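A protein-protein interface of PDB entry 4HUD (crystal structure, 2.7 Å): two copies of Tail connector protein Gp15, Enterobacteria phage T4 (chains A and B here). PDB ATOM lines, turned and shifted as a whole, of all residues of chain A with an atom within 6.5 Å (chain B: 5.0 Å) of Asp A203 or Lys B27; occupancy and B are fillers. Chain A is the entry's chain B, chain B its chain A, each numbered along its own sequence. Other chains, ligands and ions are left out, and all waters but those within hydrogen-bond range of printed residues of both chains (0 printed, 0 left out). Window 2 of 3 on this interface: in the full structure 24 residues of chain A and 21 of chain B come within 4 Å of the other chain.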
ATOM      1  N   TYR A   4      -0.205  28.304  21.707  1.00  0.00           N
ATOM      2  CA  TYR A   4       0.787  27.255  21.693  1.00  0.00           C
ATOM      3  C   TYR A   4       0.319  26.143  22.603  1.00  0.00           C
ATOM      4  O   TYR A   4      -0.381  26.385  23.569  1.00  0.00           O
ATOM      5  CB  TYR A   4       2.157  27.778  22.113  1.00  0.00           C
ATOM      6  CG  TYR A   4       2.178  28.343  23.507  1.00  0.00           C
ATOM      7  CD1 TYR A   4       2.371  27.515  24.609  1.00  0.00           C
ATOM      8  CD2 TYR A   4       1.999  29.707  23.733  1.00  0.00           C
ATOM      9  CE1 TYR A   4       2.380  28.026  25.889  1.00  0.00           C
ATOM     10  CE2 TYR A   4       2.003  30.217  25.007  1.00  0.00           C
ATOM     11  CZ  TYR A   4       2.199  29.371  26.076  1.00  0.00           C
ATOM     12  OH  TYR A   4       2.210  29.868  27.347  1.00  0.00           O
ATOM     13  N   PHE A   5       0.694  24.916  22.277  1.00  0.00           N
ATOM     14  CA  PHE A   5       0.331  23.770  23.093  1.00  0.00           C
ATOM     15  C   PHE A   5       1.078  23.807  24.435  1.00  0.00           C
ATOM     16  O   PHE A   5       2.205  23.332  24.551  1.00  0.00           O
ATOM     17  CB  PHE A   5       0.565  22.466  22.317  1.00  0.00           C
ATOM     18  CG  PHE A   5       0.353  21.230  23.129  1.00  0.00           C
ATOM     19  CD1 PHE A   5      -0.643  21.168  24.078  1.00  0.00           C
ATOM     20  CD2 PHE A   5       1.136  20.122  22.932  1.00  0.00           C
ATOM     21  CE1 PHE A   5      -0.826  20.028  24.828  1.00  0.00           C
ATOM     22  CE2 PHE A   5       0.946  18.980  23.676  1.00  0.00           C
ATOM     23  CZ  PHE A   5      -0.025  18.930  24.619  1.00  0.00           C
ATOM     24  N   ASN A   7       0.947  22.244  27.321  1.00  0.00           N
ATOM     25  CA  ASN A   7       1.409  21.021  27.977  1.00  0.00           C
ATOM     26  C   ASN A   7       2.418  20.196  27.146  1.00  0.00           C
ATOM     27  O   ASN A   7       2.786  19.073  27.516  1.00  0.00           O
ATOM     28  CB  ASN A   7       0.215  20.148  28.367  1.00  0.00           C
ATOM     29  CG  ASN A   7      -0.801  20.886  29.214  1.00  0.00           C
ATOM     30  OD1 ASN A   7      -0.458  21.645  30.114  1.00  0.00           O
ATOM     31  ND2 ASN A   7      -2.066  20.666  28.918  1.00  0.00           N
ATOM     32  N   PRO A 201       0.359  13.892  23.679  1.00  0.00           N
ATOM     33  CA  PRO A 201      -0.099  15.215  24.104  1.00  0.00           C
ATOM     34  C   PRO A 201      -1.331  15.117  24.976  1.00  0.00           C
ATOM     35  O   PRO A 201      -2.238  14.349  24.660  1.00  0.00           O
ATOM     36  CB  PRO A 201      -0.488  15.897  22.792  1.00  0.00           C
ATOM     37  CG  PRO A 201       0.186  15.173  21.758  1.00  0.00           C
ATOM     38  CD  PRO A 201       0.312  13.760  22.217  1.00  0.00           C
ATOM     39  N   VAL A 202      -1.350  15.864  26.067  1.00  0.00           N
ATOM     40  CA  VAL A 202      -2.526  15.966  26.899  1.00  0.00           C
ATOM     41  C   VAL A 202      -3.126  17.358  26.703  1.00  0.00           C
ATOM     42  O   VAL A 202      -2.558  18.344  27.147  1.00  0.00           O
ATOM     43  CB  VAL A 202      -2.149  15.718  28.359  1.00  0.00           C
ATOM     44  CG1 VAL A 202      -3.373  15.687  29.231  1.00  0.00           C
ATOM     45  CG2 VAL A 202      -1.400  14.410  28.458  1.00  0.00           C
ATOM     46  N   ASP A 203      -4.261  17.424  26.014  1.00  0.00           N
ATOM     47  CA  ASP A 203      -4.875  18.692  25.626  1.00  0.00           C
ATOM     48  C   ASP A 203      -4.947  19.721  26.760  1.00  0.00           C
ATOM     49  O   ASP A 203      -5.255  19.395  27.917  1.00  0.00           O
ATOM     50  CB  ASP A 203      -6.285  18.452  25.062  1.00  0.00           C
ATOM     51  CG  ASP A 203      -6.801  19.623  24.222  1.00  0.00           C
ATOM     52  OD1 ASP A 203      -6.442  20.789  24.510  1.00  0.00           O
ATOM     53  OD2 ASP A 203      -7.594  19.378  23.282  1.00  0.00           O
ATOM     54  N   ASP A 204      -4.690  20.972  26.402  1.00  0.00           N
ATOM     55  CA  ASP A 204      -4.723  22.065  27.356  1.00  0.00           C
ATOM     56  C   ASP A 204      -6.140  22.195  27.910  1.00  0.00           C
ATOM     57  O   ASP A 204      -6.341  22.681  29.034  1.00  0.00           O
ATOM     58  CB  ASP A 204      -4.264  23.376  26.696  1.00  0.00           C
ATOM     59  CG  ASP A 204      -2.757  23.412  26.404  1.00  0.00           C
ATOM     60  OD1 ASP A 204      -2.002  22.560  26.918  1.00  0.00           O
ATOM     61  OD2 ASP A 204      -2.326  24.303  25.641  1.00  0.00           O
ATOM     62  N   ALA A 205      -7.120  21.740  27.130  1.00  0.00           N
ATOM     63  CA  ALA A 205      -8.528  21.827  27.536  1.00  0.00           C
ATOM     64  C   ALA A 205      -8.877  20.884  28.689  1.00  0.00           C
ATOM     65  O   ALA A 205      -9.820  21.124  29.429  1.00  0.00           O
ATOM     66  CB  ALA A 205      -9.441  21.579  26.349  1.00  0.00           C
ATOM     67  N   GLU A 206      -8.082  19.836  28.850  1.00  0.00           N
ATOM     68  CA  GLU A 206      -8.224  18.859  29.924  1.00  0.00           C
ATOM     69  C   GLU A 206      -7.561  19.368  31.213  1.00  0.00           C
ATOM     70  O   GLU A 206      -7.597  18.701  32.244  1.00  0.00           O
ATOM     71  CB  GLU A 206      -7.549  17.566  29.454  1.00  0.00           C
ATOM     72  CG  GLU A 206      -7.961  16.253  30.092  1.00  0.00           C
ATOM     73  CD  GLU A 206      -7.600  15.070  29.178  1.00  0.00           C
ATOM     74  OE1 GLU A 206      -7.055  14.053  29.666  1.00  0.00           O
ATOM     75  OE2 GLU A 206      -7.857  15.172  27.956  1.00  0.00           O
ATOM     76  N   GLY A 207      -6.960  20.555  31.146  1.00  0.00           N
ATOM     77  CA  GLY A 207      -6.321  21.177  32.301  1.00  0.00           C
ATOM     78  C   GLY A 207      -4.807  21.362  32.200  1.00  0.00           C
ATOM     79  O   GLY A 207      -4.105  20.459  31.767  1.00  0.00           O
ATOM     80  N   LEU A 208      -4.317  22.524  32.636  1.00  0.00           N
ATOM     81  CA  LEU A 208      -2.899  22.905  32.542  1.00  0.00           C
ATOM     82  C   LEU A 208      -1.997  22.239  33.565  1.00  0.00           C
ATOM     83  O   LEU A 208      -2.280  22.203  34.747  1.00  0.00           O
ATOM     84  CB  LEU A 208      -2.727  24.419  32.629  1.00  0.00           C
ATOM     85  CG  LEU A 208      -2.577  25.132  31.291  1.00  0.00           C
ATOM     86  CD1 LEU A 208      -3.642  24.678  30.311  1.00  0.00           C
ATOM     87  CD2 LEU A 208      -2.602  26.630  31.448  1.00  0.00           C
ATOM     88  N   GLN B  25      -3.305  15.434  13.781  1.00  0.00           N
ATOM     89  CA  GLN B  25      -3.781  16.790  13.700  1.00  0.00           C
ATOM     90  C   GLN B  25      -3.032  17.678  14.662  1.00  0.00           C
ATOM     91  O   GLN B  25      -2.481  17.212  15.653  1.00  0.00           O
ATOM     92  CB  GLN B  25      -5.265  16.825  13.967  1.00  0.00           C
ATOM     93  CG  GLN B  25      -5.800  15.485  14.391  1.00  0.00           C
ATOM     94  CD  GLN B  25      -7.292  15.504  14.491  1.00  0.00           C
ATOM     95  OE1 GLN B  25      -7.985  15.461  13.472  1.00  0.00           O
ATOM     96  NE2 GLN B  25      -7.811  15.598  15.717  1.00  0.00           N
ATOM     97  N   ILE B  26      -2.991  18.962  14.353  1.00  0.00           N
ATOM     98  CA  ILE B  26      -2.457  19.927  15.287  1.00  0.00           C
ATOM     99  C   ILE B  26      -3.554  20.894  15.735  1.00  0.00           C
ATOM    100  O   ILE B  26      -4.418  21.284  14.938  1.00  0.00           O
ATOM    101  CB  ILE B  26      -1.324  20.718  14.657  1.00  0.00           C
ATOM    102  CG1 ILE B  26      -1.799  21.358  13.354  1.00  0.00           C
ATOM    103  CG2 ILE B  26      -0.175  19.802  14.379  1.00  0.00           C
ATOM    104  CD1 ILE B  26      -1.139  22.675  13.035  1.00  0.00           C
ATOM    105  N   LYS B  27      -3.526  21.257  17.017  1.00  0.00           N
ATOM    106  CA  LYS B  27      -4.445  22.263  17.558  1.00  0.00           C
ATOM    107  C   LYS B  27      -3.894  23.657  17.268  1.00  0.00           C
ATOM    108  O   LYS B  27      -2.718  23.936  17.468  1.00  0.00           O
ATOM    109  CB  LYS B  27      -4.651  22.074  19.069  1.00  0.00           C
ATOM    110  CG  LYS B  27      -5.567  23.113  19.736  1.00  0.00           C
ATOM    111  CD  LYS B  27      -5.865  22.779  21.204  1.00  0.00           C
ATOM    112  CE  LYS B  27      -6.484  23.986  21.938  1.00  0.00           C
ATOM    113  NZ  LYS B  27      -6.514  23.918  23.445  1.00  0.00           N
ATOM    114  N   ARG B  28      -4.777  24.539  16.850  1.00  0.00           N
ATOM    115  CA  ARG B  28      -4.450  25.867  16.387  1.00  0.00           C
ATOM    116  C   ARG B  28      -5.503  26.808  17.000  1.00  0.00           C
ATOM    117  O   ARG B  28      -6.627  26.904  16.485  1.00  0.00           O
ATOM    118  CB  ARG B  28      -4.524  25.835  14.860  1.00  0.00           C
ATOM    119  CG  ARG B  28      -4.021  27.033  14.112  1.00  0.00           C
ATOM    120  CD  ARG B  28      -2.587  27.408  14.501  1.00  0.00           C
ATOM    121  NE  ARG B  28      -1.524  26.702  13.788  1.00  0.00           N
ATOM    122  CZ  ARG B  28      -1.279  26.808  12.486  1.00  0.00           C
ATOM    123  NH1 ARG B  28      -2.065  27.545  11.707  1.00  0.00           N
ATOM    124  NH2 ARG B  28      -0.258  26.145  11.962  1.00  0.00           N
ATOM    125  N   GLN B  29      -5.159  27.481  18.108  1.00  0.00           N
ATOM    126  CA  GLN B  29      -6.150  28.281  18.871  1.00  0.00           C
ATOM    127  C   GLN B  29      -6.597  29.569  18.172  1.00  0.00           C
ATOM    128  O   GLN B  29      -5.797  30.456  17.923  1.00  0.00           O
ATOM    129  CB  GLN B  29      -5.649  28.642  20.271  1.00  0.00           C
ATOM    130  CG  GLN B  29      -4.933  27.538  21.016  1.00  0.00           C
ATOM    131  CD  GLN B  29      -4.243  28.081  22.257  1.00  0.00           C
ATOM    132  OE1 GLN B  29      -4.663  29.097  22.812  1.00  0.00           O
ATOM    133  NE2 GLN B  29      -3.167  27.423  22.683  1.00  0.00           N
ATOM    134  N   ASP B  34     -10.970  26.906  19.021  1.00  0.00           N
ATOM    135  CA  ASP B  34      -9.905  26.025  18.570  1.00  0.00           C
ATOM    136  C   ASP B  34     -10.168  25.398  17.201  1.00  0.00           C
ATOM    137  O   ASP B  34     -11.239  24.867  16.955  1.00  0.00           O
ATOM    138  CB  ASP B  34      -9.703  24.910  19.592  1.00  0.00           C
ATOM    139  CG  ASP B  34      -9.541  25.434  20.993  1.00  0.00           C
ATOM    140  OD1 ASP B  34      -8.778  26.406  21.183  1.00  0.00           O
ATOM    141  OD2 ASP B  34     -10.195  24.885  21.905  1.00  0.00           O
ATOM    142  N   LYS B  35      -9.183  25.459  16.309  1.00  0.00           N
ATOM    143  CA  LYS B  35      -9.302  24.753  15.039  1.00  0.00           C
ATOM    144  C   LYS B  35      -8.294  23.616  14.998  1.00  0.00           C
ATOM    145  O   LYS B  35      -7.139  23.822  15.308  1.00  0.00           O
ATOM    146  CB  LYS B  35      -9.082  25.697  13.859  1.00  0.00           C
ATOM    147  CG  LYS B  35      -8.834  24.965  12.557  1.00  0.00           C
ATOM    148  CD  LYS B  35      -8.668  25.923  11.387  1.00  0.00           C
ATOM    149  CE  LYS B  35      -9.997  26.510  10.953  1.00  0.00           C
ATOM    150  NZ  LYS B  35      -9.846  27.167   9.623  1.00  0.00           N
ATOM    151  N   PHE B  36      -8.743  22.418  14.641  1.00  0.00           N
ATOM    152  CA  PHE B  36      -7.843  21.282  14.544  1.00  0.00           C
ATOM    153  C   PHE B  36      -7.546  21.023  13.083  1.00  0.00           C
ATOM    154  O   PHE B  36      -8.449  20.820  12.301  1.00  0.00           O
ATOM    155  CB  PHE B  36      -8.469  20.050  15.194  1.00  0.00           C
ATOM    156  CG  PHE B  36      -8.410  20.072  16.685  1.00  0.00           C
ATOM    157  CD1 PHE B  36      -9.495  20.511  17.433  1.00  0.00           C
ATOM    158  CD2 PHE B  36      -7.254  19.705  17.349  1.00  0.00           C
ATOM    159  CE1 PHE B  36      -9.434  20.555  18.816  1.00  0.00           C
ATOM    160  CE2 PHE B  36      -7.173  19.746  18.734  1.00  0.00           C
ATOM    161  CZ  PHE B  36      -8.267  20.170  19.471  1.00  0.00           C
ATOM    162  N   ASP B 128       5.910  25.154  17.459  1.00  0.00           N
ATOM    163  CA  ASP B 128       4.739  24.602  18.148  1.00  0.00           C
ATOM    164  C   ASP B 128       4.048  23.511  17.345  1.00  0.00           C
ATOM    165  O   ASP B 128       3.798  22.411  17.854  1.00  0.00           O
ATOM    166  CB  ASP B 128       3.746  25.734  18.472  1.00  0.00           C
ATOM    167  CG  ASP B 128       2.527  25.246  19.240  1.00  0.00           C
ATOM    168  OD1 ASP B 128       2.716  24.812  20.398  1.00  0.00           O
ATOM    169  OD2 ASP B 128       1.393  25.293  18.693  1.00  0.00           O
ATOM    170  N   GLN B 132       3.810  19.504  18.502  1.00  0.00           N
ATOM    171  CA  GLN B 132       2.558  18.766  18.527  1.00  0.00           C
ATOM    172  C   GLN B 132       2.649  17.472  17.742  1.00  0.00           C
ATOM    173  O   GLN B 132       2.460  16.367  18.302  1.00  0.00           O
ATOM    174  CB  GLN B 132       1.424  19.642  17.991  1.00  0.00           C
ATOM    175  CG  GLN B 132       0.891  20.631  19.014  1.00  0.00           C
ATOM    176  CD  GLN B 132      -0.237  21.477  18.462  1.00  0.00           C
ATOM    177  OE1 GLN B 132      -1.363  20.993  18.248  1.00  0.00           O
ATOM    178  NE2 GLN B 132       0.043  22.769  18.261  1.00  0.00           N
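No position is printed for both chains.
Tyr A4 touches Asp B128 (CA to OD1, 3.4 Å).
Gln B132 touches Phe A5.
Phe B36 touches Asp A203.
CB of Asp A204 touches NZ of Lys B27, at 3.99 Å.
NZ of Lys B27 is in salt-bridge range of OD1 of Asp A203 (3.3 Å).
O of Tyr A4 sits at hydrogen-bond distance from NE2 of Gln B29.
The side-chain carboxylate (OD1) of Asp B128 sits at hydrogen-bond distance from the backbone NH (N) of Phe A5 (2.8 Å).
Val A202 touches none of the printed residues of chain B.
Asp A203 touches two residues of chain B.
Printed residues of chain A within 4 Å of Lys B27: Asp A203 (3.3 Å) and Asp A204 (3.99 Å).
Arg B28 touches none of the printed residues of chain A.
Printed residues of chain A within 4 Å of Gln B29: Tyr A4.
Printed residues of chain A within 4 Å of Gln B132: Phe A5.
The nearest printed residue of chain B that does not touch Asp A203 is Asp B34 (6.1 Å).
The nearest printed residue of chain A that does not touch Lys B27 is Ala A205 (4.3 Å).
The nearest printed residue of chain A that does not touch Phe B36 is Ala A205 (7.1 Å).
OE1 of Gln B132 sits at hydrogen-bond distance from N of Lys B27 (2.5 Å).
The side-chain carboxylate (OD2) of Asp B128 sits at hydrogen-bond distance from the side-chain amide nitrogen (NE2) of Gln B132, 2.9 Å away.
ND2 of Asn A7 sits at hydrogen-bond distance from OD1 of Asp A204, at 2.8 Å.
N of Ala A205 sits at hydrogen-bond distance from OD1 of Asp A203 (2.9 Å).
Of the 11 printed residues of chain A, 4 touch a printed residue of chain B.
Hydrophobic or aromatic side chains of chain A within 4 Å of the printed part of chain B: Tyr A4 and Phe A5.
Hydrophobic or aromatic side chains of chain B that line the printed part of chain A: Phe B36.
Among the printed residues, Asp or Glu carboxylates within 4 Å of a Lys or Arg side-chain nitrogen of the other chain: Asp A203 with Lys B27 (3.3 Å).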
